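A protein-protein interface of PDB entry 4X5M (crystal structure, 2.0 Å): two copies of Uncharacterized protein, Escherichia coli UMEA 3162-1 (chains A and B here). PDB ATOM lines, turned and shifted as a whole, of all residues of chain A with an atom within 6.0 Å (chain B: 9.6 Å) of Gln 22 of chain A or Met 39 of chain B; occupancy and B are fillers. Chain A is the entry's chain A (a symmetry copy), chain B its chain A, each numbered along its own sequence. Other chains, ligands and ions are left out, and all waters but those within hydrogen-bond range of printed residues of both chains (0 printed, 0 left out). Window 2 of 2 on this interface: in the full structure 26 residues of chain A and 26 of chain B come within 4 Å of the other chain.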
ATOM      1  N   PHE A  14       9.117 -20.822  37.899  1.00  0.00           N
ATOM      2  CA  PHE A  14       8.418 -21.386  36.750  1.00  0.00           C
ATOM      3  C   PHE A  14       8.757 -20.700  35.429  1.00  0.00           C
ATOM      4  O   PHE A  14       8.943 -21.372  34.421  1.00  0.00           O
ATOM      5  CB  PHE A  14       6.907 -21.350  36.980  1.00  0.00           C
ATOM      6  CG  PHE A  14       6.399 -22.497  37.804  1.00  0.00           C
ATOM      7  CD1 PHE A  14       6.159 -23.729  37.220  1.00  0.00           C
ATOM      8  CD2 PHE A  14       6.170 -22.346  39.160  1.00  0.00           C
ATOM      9  CE1 PHE A  14       5.696 -24.791  37.973  1.00  0.00           C
ATOM     10  CE2 PHE A  14       5.708 -23.405  39.919  1.00  0.00           C
ATOM     11  CZ  PHE A  14       5.470 -24.627  39.325  1.00  0.00           C
ATOM     12  N   ALA A  18      11.157 -22.816  32.820  1.00  0.00           N
ATOM     13  CA  ALA A  18      10.239 -23.343  31.813  1.00  0.00           C
ATOM     14  C   ALA A  18      10.969 -23.689  30.523  1.00  0.00           C
ATOM     15  O   ALA A  18      10.839 -24.797  30.004  1.00  0.00           O
ATOM     16  CB  ALA A  18       9.128 -22.346  31.527  1.00  0.00           C
ATOM     17  N   PHE A  19      11.734 -22.732  30.009  1.00  0.00           N
ATOM     18  CA  PHE A  19      12.438 -22.911  28.745  1.00  0.00           C
ATOM     19  C   PHE A  19      13.947 -22.971  28.937  1.00  0.00           C
ATOM     20  O   PHE A  19      14.709 -22.869  27.976  1.00  0.00           O
ATOM     21  CB  PHE A  19      12.079 -21.786  27.776  1.00  0.00           C
ATOM     22  CG  PHE A  19      10.617 -21.719  27.446  1.00  0.00           C
ATOM     23  CD1 PHE A  19      10.068 -22.570  26.502  1.00  0.00           C
ATOM     24  CD2 PHE A  19       9.791 -20.807  28.080  1.00  0.00           C
ATOM     25  CE1 PHE A  19       8.723 -22.514  26.196  1.00  0.00           C
ATOM     26  CE2 PHE A  19       8.446 -20.744  27.778  1.00  0.00           C
ATOM     27  CZ  PHE A  19       7.911 -21.599  26.834  1.00  0.00           C
ATOM     28  N   ALA A  20      14.374 -23.131  30.186  1.00  0.00           N
ATOM     29  CA  ALA A  20      15.790 -23.290  30.503  1.00  0.00           C
ATOM     30  C   ALA A  20      16.454 -24.482  29.792  1.00  0.00           C
ATOM     31  O   ALA A  20      17.602 -24.365  29.367  1.00  0.00           O
ATOM     32  CB  ALA A  20      15.982 -23.407  32.014  1.00  0.00           C
ATOM     33  N   PRO A  21      15.752 -25.632  29.667  1.00  0.00           N
ATOM     34  CA  PRO A  21      16.381 -26.725  28.913  1.00  0.00           C
ATOM     35  C   PRO A  21      16.741 -26.369  27.468  1.00  0.00           C
ATOM     36  O   PRO A  21      17.651 -26.982  26.909  1.00  0.00           O
ATOM     37  CB  PRO A  21      15.315 -27.823  28.943  1.00  0.00           C
ATOM     38  CG  PRO A  21      14.594 -27.590  30.212  1.00  0.00           C
ATOM     39  CD  PRO A  21      14.534 -26.097  30.362  1.00  0.00           C
ATOM     40  N   GLN A  22      16.043 -25.403  26.878  1.00  0.00           N
ATOM     41  CA  GLN A  22      16.354 -24.960  25.521  1.00  0.00           C
ATOM     42  C   GLN A  22      17.705 -24.251  25.463  1.00  0.00           C
ATOM     43  O   GLN A  22      18.514 -24.510  24.571  1.00  0.00           O
ATOM     44  CB  GLN A  22      15.255 -24.036  24.984  1.00  0.00           C
ATOM     45  CG  GLN A  22      13.941 -24.736  24.666  1.00  0.00           C
ATOM     46  CD  GLN A  22      13.004 -23.867  23.848  1.00  0.00           C
ATOM     47  OE1 GLN A  22      13.212 -22.660  23.720  1.00  0.00           O
ATOM     48  NE2 GLN A  22      11.970 -24.478  23.281  1.00  0.00           N
ATOM     49  N   SER A  23      17.940 -23.354  26.416  1.00  0.00           N
ATOM     50  CA  SER A  23      19.204 -22.628  26.497  1.00  0.00           C
ATOM     51  C   SER A  23      20.358 -23.568  26.822  1.00  0.00           C
ATOM     52  O   SER A  23      21.440 -23.459  26.245  1.00  0.00           O
ATOM     53  CB  SER A  23      19.123 -21.517  27.546  1.00  0.00           C
ATOM     54  OG  SER A  23      18.176 -20.531  27.172  1.00  0.00           O
ATOM     55  N   ILE A  24      20.118 -24.488  27.752  1.00  0.00           N
ATOM     56  CA  ILE A  24      21.120 -25.473  28.143  1.00  0.00           C
ATOM     57  C   ILE A  24      21.520 -26.338  26.951  1.00  0.00           C
ATOM     58  O   ILE A  24      22.703 -26.605  26.734  1.00  0.00           O
ATOM     59  CB  ILE A  24      20.612 -26.373  29.288  1.00  0.00           C
ATOM     60  CG1 ILE A  24      20.368 -25.545  30.551  1.00  0.00           C
ATOM     61  CG2 ILE A  24      21.605 -27.491  29.574  1.00  0.00           C
ATOM     62  CD1 ILE A  24      19.742 -26.330  31.688  1.00  0.00           C
ATOM     63  N   LYS A  25      20.526 -26.763  26.177  1.00  0.00           N
ATOM     64  CA  LYS A  25      20.767 -27.548  24.971  1.00  0.00           C
ATOM     65  C   LYS A  25      21.611 -26.769  23.967  1.00  0.00           C
ATOM     66  O   LYS A  25      22.519 -27.319  23.344  1.00  0.00           O
ATOM     67  CB  LYS A  25      19.445 -27.964  24.323  1.00  0.00           C
ATOM     68  CG  LYS A  25      19.609 -28.870  23.113  1.00  0.00           C
ATOM     69  CD  LYS A  25      18.355 -28.886  22.255  1.00  0.00           C
ATOM     70  CE  LYS A  25      18.018 -30.297  21.802  1.00  0.00           C
ATOM     71  NZ  LYS A  25      19.211 -31.011  21.260  1.00  0.00           N
ATOM     72  N   THR A  26      21.296 -25.486  23.815  1.00  0.00           N
ATOM     73  CA  THR A  26      22.028 -24.613  22.904  1.00  0.00           C
ATOM     74  C   THR A  26      23.479 -24.466  23.346  1.00  0.00           C
ATOM     75  O   THR A  26      24.398 -24.533  22.529  1.00  0.00           O
ATOM     76  CB  THR A  26      21.380 -23.215  22.812  1.00  0.00           C
ATOM     77  OG1 THR A  26      20.050 -23.339  22.294  1.00  0.00           O
ATOM     78  CG2 THR A  26      22.190 -22.304  21.901  1.00  0.00           C
ATOM     79  N   ILE A  27      23.677 -24.272  24.645  1.00  0.00           N
ATOM     80  CA  ILE A  27      25.015 -24.158  25.213  1.00  0.00           C
ATOM     81  C   ILE A  27      25.793 -25.461  25.035  1.00  0.00           C
ATOM     82  O   ILE A  27      26.981 -25.452  24.707  1.00  0.00           O
ATOM     83  CB  ILE A  27      24.957 -23.785  26.710  1.00  0.00           C
ATOM     84  CG1 ILE A  27      24.361 -22.385  26.884  1.00  0.00           C
ATOM     85  CG2 ILE A  27      26.340 -23.850  27.342  1.00  0.00           C
ATOM     86  CD1 ILE A  27      24.201 -21.960  28.329  1.00  0.00           C
ATOM     87  N   PHE B  19      11.253 -11.085  21.700  1.00  0.00           N
ATOM     88  CA  PHE B  19      10.894 -12.304  20.985  1.00  0.00           C
ATOM     89  C   PHE B  19       9.409 -12.348  20.646  1.00  0.00           C
ATOM     90  O   PHE B  19       8.880 -13.394  20.271  1.00  0.00           O
ATOM     91  CB  PHE B  19      11.278 -13.533  21.807  1.00  0.00           C
ATOM     92  CG  PHE B  19      12.746 -13.626  22.100  1.00  0.00           C
ATOM     93  CD1 PHE B  19      13.625 -14.114  21.148  1.00  0.00           C
ATOM     94  CD2 PHE B  19      13.249 -13.225  23.326  1.00  0.00           C
ATOM     95  CE1 PHE B  19      14.977 -14.200  21.412  1.00  0.00           C
ATOM     96  CE2 PHE B  19      14.599 -13.310  23.597  1.00  0.00           C
ATOM     97  CZ  PHE B  19      15.465 -13.798  22.639  1.00  0.00           C
ATOM     98  N   GLN B  22       8.256 -13.742  17.288  1.00  0.00           N
ATOM     99  CA  GLN B  22       8.194 -15.199  17.209  1.00  0.00           C
ATOM    100  C   GLN B  22       6.796 -15.716  17.539  1.00  0.00           C
ATOM    101  O   GLN B  22       6.264 -16.580  16.840  1.00  0.00           O
ATOM    102  CB  GLN B  22       9.224 -15.839  18.147  1.00  0.00           C
ATOM    103  CG  GLN B  22      10.671 -15.679  17.701  1.00  0.00           C
ATOM    104  CD  GLN B  22      11.617 -16.587  18.465  1.00  0.00           C
ATOM    105  OE1 GLN B  22      11.252 -17.157  19.493  1.00  0.00           O
ATOM    106  NE2 GLN B  22      12.837 -16.732  17.961  1.00  0.00           N
ATOM    107  N   GLU B  33       5.183 -26.594  15.573  1.00  0.00           N
ATOM    108  CA  GLU B  33       6.138 -27.696  15.632  1.00  0.00           C
ATOM    109  C   GLU B  33       7.284 -27.378  16.589  1.00  0.00           C
ATOM    110  O   GLU B  33       7.886 -26.306  16.518  1.00  0.00           O
ATOM    111  CB  GLU B  33       6.689 -28.013  14.238  1.00  0.00           C
ATOM    112  CG  GLU B  33       5.743 -28.822  13.360  1.00  0.00           C
ATOM    113  N   GLY B  34       7.576 -28.314  17.489  1.00  0.00           N
ATOM    114  CA  GLY B  34       8.667 -28.148  18.432  1.00  0.00           C
ATOM    115  C   GLY B  34       8.222 -27.579  19.764  1.00  0.00           C
ATOM    116  O   GLY B  34       8.883 -27.777  20.786  1.00  0.00           O
ATOM    117  N   ILE B  35       7.097 -26.870  19.755  1.00  0.00           N
ATOM    118  CA  ILE B  35       6.568 -26.256  20.968  1.00  0.00           C
ATOM    119  C   ILE B  35       6.124 -27.307  21.981  1.00  0.00           C
ATOM    120  O   ILE B  35       5.297 -28.167  21.676  1.00  0.00           O
ATOM    121  CB  ILE B  35       5.381 -25.326  20.655  1.00  0.00           C
ATOM    122  CG1 ILE B  35       5.835 -24.168  19.766  1.00  0.00           C
ATOM    123  CG2 ILE B  35       4.762 -24.802  21.942  1.00  0.00           C
ATOM    124  CD1 ILE B  35       4.736 -23.184  19.431  1.00  0.00           C
ATOM    125  N   SER B  36       6.683 -27.233  23.184  1.00  0.00           N
ATOM    126  CA  SER B  36       6.317 -28.153  24.254  1.00  0.00           C
ATOM    127  C   SER B  36       5.128 -27.637  25.052  1.00  0.00           C
ATOM    128  O   SER B  36       5.156 -26.522  25.577  1.00  0.00           O
ATOM    129  CB  SER B  36       7.501 -28.392  25.188  1.00  0.00           C
ATOM    130  OG  SER B  36       7.082 -29.008  26.392  1.00  0.00           O
ATOM    131  N   VAL B  37       4.087 -28.458  25.140  1.00  0.00           N
ATOM    132  CA  VAL B  37       2.903 -28.123  25.923  1.00  0.00           C
ATOM    133  C   VAL B  37       3.260 -27.944  27.395  1.00  0.00           C
ATOM    134  O   VAL B  37       2.825 -26.986  28.036  1.00  0.00           O
ATOM    135  CB  VAL B  37       1.815 -29.207  25.784  1.00  0.00           C
ATOM    136  CG1 VAL B  37       0.652 -28.923  26.723  1.00  0.00           C
ATOM    137  CG2 VAL B  37       1.334 -29.293  24.343  1.00  0.00           C
ATOM    138  N   VAL B  38       4.068 -28.862  27.918  1.00  0.00           N
ATOM    139  CA  VAL B  38       4.480 -28.829  29.321  1.00  0.00           C
ATOM    140  C   VAL B  38       5.240 -27.550  29.664  1.00  0.00           C
ATOM    141  O   VAL B  38       4.984 -26.924  30.694  1.00  0.00           O
ATOM    142  CB  VAL B  38       5.359 -30.048  29.675  1.00  0.00           C
ATOM    143  CG1 VAL B  38       5.935 -29.906  31.079  1.00  0.00           C
ATOM    144  CG2 VAL B  38       4.556 -31.332  29.555  1.00  0.00           C
ATOM    145  N   MET B  39       6.167 -27.158  28.794  1.00  0.00           N
ATOM    146  CA  MET B  39       6.964 -25.958  29.028  1.00  0.00           C
ATOM    147  C   MET B  39       6.095 -24.701  29.054  1.00  0.00           C
ATOM    148  O   MET B  39       6.316 -23.805  29.868  1.00  0.00           O
ATOM    149  CB  MET B  39       8.062 -25.818  27.966  1.00  0.00           C
ATOM    150  CG  MET B  39       9.160 -26.867  28.065  1.00  0.00           C
ATOM    151  SD  MET B  39      10.707 -26.363  27.277  1.00  0.00           S
ATOM    152  CE  MET B  39      10.166 -26.059  25.601  1.00  0.00           C
ATOM    153  N   TYR B  40       5.101 -24.639  28.172  1.00  0.00           N
ATOM    154  CA  TYR B  40       4.230 -23.470  28.108  1.00  0.00           C
ATOM    155  C   TYR B  40       3.264 -23.410  29.287  1.00  0.00           C
ATOM    156  O   TYR B  40       2.922 -22.325  29.759  1.00  0.00           O
ATOM    157  CB  TYR B  40       3.458 -23.444  26.786  1.00  0.00           C
ATOM    158  CG  TYR B  40       4.066 -22.501  25.775  1.00  0.00           C
ATOM    159  CD1 TYR B  40       5.146 -22.892  24.996  1.00  0.00           C
ATOM    160  CD2 TYR B  40       3.572 -21.213  25.614  1.00  0.00           C
ATOM    161  CE1 TYR B  40       5.714 -22.031  24.075  1.00  0.00           C
ATOM    162  CE2 TYR B  40       4.132 -20.342  24.696  1.00  0.00           C
ATOM    163  CZ  TYR B  40       5.202 -20.758  23.929  1.00  0.00           C
ATOM    164  OH  TYR B  40       5.765 -19.897  23.014  1.00  0.00           O
ATOM    165  N   ILE B  41       2.826 -24.571  29.762  1.00  0.00           N
ATOM    166  CA  ILE B  41       1.973 -24.629  30.942  1.00  0.00           C
ATOM    167  C   ILE B  41       2.755 -24.175  32.171  1.00  0.00           C
ATOM    168  O   ILE B  41       2.246 -23.416  32.999  1.00  0.00           O
ATOM    169  CB  ILE B  41       1.406 -26.045  31.173  1.00  0.00           C
ATOM    170  CG1 ILE B  41       0.438 -26.414  30.048  1.00  0.00           C
ATOM    171  CG2 ILE B  41       0.697 -26.130  32.515  1.00  0.00           C
ATOM    172  CD1 ILE B  41      -0.181 -27.787  30.198  1.00  0.00           C
ATOM    173  N   MET B  42       3.998 -24.635  32.280  1.00  0.00           N
ATOM    174  CA  MET B  42       4.892 -24.177  33.338  1.00  0.00           C
ATOM    175  C   MET B  42       5.121 -22.673  33.236  1.00  0.00           C
ATOM    176  O   MET B  42       5.089 -21.957  34.238  1.00  0.00           O
ATOM    177  CB  MET B  42       6.234 -24.910  33.277  1.00  0.00           C
ATOM    178  CG  MET B  42       6.230 -26.303  33.874  1.00  0.00           C
ATOM    179  SD  MET B  42       7.896 -26.992  33.924  1.00  0.00           S
ATOM    180  CE  MET B  42       8.772 -25.677  34.772  1.00  0.00           C
ATOM    181  N   PHE B  43       5.355 -22.206  32.013  1.00  0.00           N
ATOM    182  CA  PHE B  43       5.611 -20.794  31.753  1.00  0.00           C
ATOM    183  C   PHE B  43       4.414 -19.932  32.138  1.00  0.00           C
ATOM    184  O   PHE B  43       4.565 -18.910  32.807  1.00  0.00           O
ATOM    185  CB  PHE B  43       5.959 -20.582  30.278  1.00  0.00           C
ATOM    186  CG  PHE B  43       6.324 -19.164  29.936  1.00  0.00           C
ATOM    187  CD1 PHE B  43       7.490 -18.600  30.422  1.00  0.00           C
ATOM    188  CD2 PHE B  43       5.507 -18.403  29.115  1.00  0.00           C
ATOM    189  CE1 PHE B  43       7.831 -17.299  30.106  1.00  0.00           C
ATOM    190  CE2 PHE B  43       5.843 -17.102  28.794  1.00  0.00           C
ATOM    191  CZ  PHE B  43       7.007 -16.550  29.290  1.00  0.00           C
ATOM    192  N   LEU B  44       3.228 -20.354  31.711  1.00  0.00           N
ATOM    193  CA  LEU B  44       2.000 -19.619  31.996  1.00  0.00           C
ATOM    194  C   LEU B  44       1.673 -19.628  33.486  1.00  0.00           C
ATOM    195  O   LEU B  44       1.144 -18.652  34.017  1.00  0.00           O
ATOM    196  CB  LEU B  44       0.831 -20.197  31.196  1.00  0.00           C
ATOM    197  CG  LEU B  44       0.793 -19.804  29.718  1.00  0.00           C
ATOM    198  CD1 LEU B  44      -0.309 -20.551  28.989  1.00  0.00           C
ATOM    199  CD2 LEU B  44       0.604 -18.304  29.584  1.00  0.00           C
ATOM    200  N   THR B  45       1.987 -20.736  34.152  1.00  0.00           N
ATOM    201  CA  THR B  45       1.805 -20.837  35.596  1.00  0.00           C
ATOM    202  C   THR B  45       2.610 -19.751  36.304  1.00  0.00           C
ATOM    203  O   THR B  45       2.126 -19.107  37.237  1.00  0.00           O
ATOM    204  CB  THR B  45       2.227 -22.223  36.127  1.00  0.00           C
ATOM    205  OG1 THR B  45       1.385 -23.231  35.554  1.00  0.00           O
ATOM    206  CG2 THR B  45       2.108 -22.279  37.641  1.00  0.00           C
ATOM    207  N   GLY B  46       3.839 -19.545  35.841  1.00  0.00           N
ATOM    208  CA  GLY B  46       4.693 -18.510  36.391  1.00  0.00           C
ATOM    209  C   GLY B  46       4.209 -17.115  36.044  1.00  0.00           C
ATOM    210  O   GLY B  46       4.264 -16.209  36.877  1.00  0.00           O
ATOM    211  N   VAL B  47       3.736 -16.942  34.811  1.00  0.00           N
ATOM    212  CA  VAL B  47       3.225 -15.652  34.353  1.00  0.00           C
ATOM    213  C   VAL B  47       2.047 -15.195  35.205  1.00  0.00           C
ATOM    214  O   VAL B  47       1.991 -14.043  35.638  1.00  0.00           O
ATOM    215  CB  VAL B  47       2.795 -15.706  32.871  1.00  0.00           C
ATOM    216  CG1 VAL B  47       2.023 -14.450  32.490  1.00  0.00           C
ATOM    217  CG2 VAL B  47       4.007 -15.878  31.970  1.00  0.00           C
ATOM    218  N   ALA B  73       1.439 -15.611  24.978  1.00  0.00           N
ATOM    219  CA  ALA B  73       1.742 -17.009  25.271  1.00  0.00           C
ATOM    220  C   ALA B  73       0.504 -17.903  25.238  1.00  0.00           C
ATOM    221  O   ALA B  73       0.558 -19.023  24.733  1.00  0.00           O
ATOM    222  CB  ALA B  73       2.431 -17.121  26.625  1.00  0.00           C
ATOM    223  N   VAL B  76      -0.638 -19.050  21.806  1.00  0.00           N
ATOM    224  CA  VAL B  76       0.332 -20.016  21.297  1.00  0.00           C
ATOM    225  C   VAL B  76       0.038 -21.420  21.825  1.00  0.00           C
ATOM    226  O   VAL B  76       0.058 -22.394  21.069  1.00  0.00           O
ATOM    227  CB  VAL B  76       1.775 -19.616  21.667  1.00  0.00           C
ATOM    228  CG1 VAL B  76       2.744 -20.751  21.365  1.00  0.00           C
ATOM    229  CG2 VAL B  76       2.182 -18.355  20.922  1.00  0.00           C
ATOM    230  N   LEU B  77      -0.247 -21.520  23.120  1.00  0.00           N
ATOM    231  CA  LEU B  77      -0.577 -22.808  23.724  1.00  0.00           C
ATOM    232  C   LEU B  77      -1.895 -23.348  23.174  1.00  0.00           C
ATOM    233  O   LEU B  77      -2.022 -24.547  22.918  1.00  0.00           O
ATOM    234  CB  LEU B  77      -0.646 -22.695  25.250  1.00  0.00           C
ATOM    235  CG  LEU B  77      -1.001 -23.986  25.998  1.00  0.00           C
ATOM    236  CD1 LEU B  77      -0.081 -25.124  25.583  1.00  0.00           C
ATOM    237  CD2 LEU B  77      -0.943 -23.780  27.502  1.00  0.00           C
ATOM    238  N   THR B  80      -1.317 -24.729  19.828  1.00  0.00           N
ATOM    239  CA  THR B  80      -0.518 -25.937  20.013  1.00  0.00           C
ATOM    240  C   THR B  80      -1.393 -27.127  20.394  1.00  0.00           C
ATOM    241  O   THR B  80      -1.240 -28.223  19.853  1.00  0.00           O
ATOM    242  CB  THR B  80       0.564 -25.743  21.095  1.00  0.00           C
ATOM    243  OG1 THR B  80       1.448 -24.684  20.706  1.00  0.00           O
ATOM    244  CG2 THR B  80       1.370 -27.020  21.282  1.00  0.00           C
ATOM    245  N   ARG B  84      -2.126 -30.392  18.174  1.00  0.00           N
ATOM    246  CA  ARG B  84      -1.808 -31.671  18.802  1.00  0.00           C
ATOM    247  C   ARG B  84      -2.954 -32.669  18.656  1.00  0.00           C
ATOM    248  O   ARG B  84      -2.731 -33.859  18.431  1.00  0.00           O
ATOM    249  CB  ARG B  84      -1.482 -31.472  20.286  1.00  0.00           C
ATOM    250  CG  ARG B  84      -1.467 -32.761  21.097  1.00  0.00           C
ATOM    251  CD  ARG B  84      -1.909 -32.522  22.534  1.00  0.00           C
ATOM    252  NE  ARG B  84      -0.796 -32.175  23.414  1.00  0.00           N
ATOM    253  CZ  ARG B  84      -0.180 -33.039  24.214  1.00  0.00           C
ATOM    254  NH1 ARG B  84      -0.571 -34.306  24.252  1.00  0.00           N
ATOM    255  NH2 ARG B  84       0.823 -32.637  24.981  1.00  0.00           N
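Printed residues of chain A that touch a printed residue of chain B: Phe 14, Ala 18, Phe 19 and Gln 22.
Among the printed residues, 8 pairs touch across the chains.
Printed residues of chain B within 4 Å of Ala 18 of chain A: Met 39 (3.1 Å) and Phe 43 (3.8 Å).
Of chain B, only Met 39 (3.6 Å), Tyr 40 (3.6 Å) and Phe 43 (3.4 Å) come within 4 Å of Phe 19 of chain A.
Ala 20 of chain A touches none of the printed residues of chain B.
Of chain B, only Met 39 comes within 4 Å of Gln 22 of chain A.
No residue of chain B comes within 4 Å of Ser 23 of chain A.
Of chain A, only Ala 18 (3.1 Å), Phe 19 (3.6 Å) and Gln 22 (3.3 Å) come within 4 Å of Met 39 of chain B.
Of the printed residues of chain A, Met 42 of chain B touches Phe 14.
Printed residues of chain A within 4 Å of Phe 43 of chain B: Ala 18 and Phe 19.
Printed residues of chain A within 4 Å of Gly 46 of chain B: Phe 14.
The nearest residue of chain B that does not touch Gln 22 of chain A is Gly 34 of chain B (5.2 Å).
The nearest printed residue of chain A that does not touch Phe 43 of chain B is Phe 14 of chain A (4.3 Å).
CB of Phe 14 of chain A touches O of Met 42 of chain B, 3.3 Å away.
CB of Phe 14 of chain A touches CA of Gly 46 of chain B, 3.6 Å away.
N of Phe 43 of chain B touches CB of Ala 18 of chain A (3.8 Å).
Phe 19 of chain A touches Met 39 of chain B (CD1 to CE, 3.6 Å).
CZ of Phe 19 of chain A touches CE1 of Tyr 40 of chain B, at 3.6 Å.
Phe 43 of chain B touches Phe 19 of chain A (CG to CE2, 3.4 Å).
Gln 22 of chain A touches Met 39 of chain B.
O of Ala 18 of chain A sits close to SD of Met 39 of chain B, at 3.1 Å.
Positions printed for both chains: 19 and 22.
Of the 8 pairs that touch across the chains among the printed residues, none has its exchanged pair printed and touching as well.
OG of Ser 36 of chain B is in hydrogen-bond range of N of Met 39 of chain B (3.2 Å).
The backbone carbonyl oxygen (O) of Gln 22 of chain A is in hydrogen-bond range of the side-chain hydroxyl (OG1) of Thr 26 of chain A (3.0 Å).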
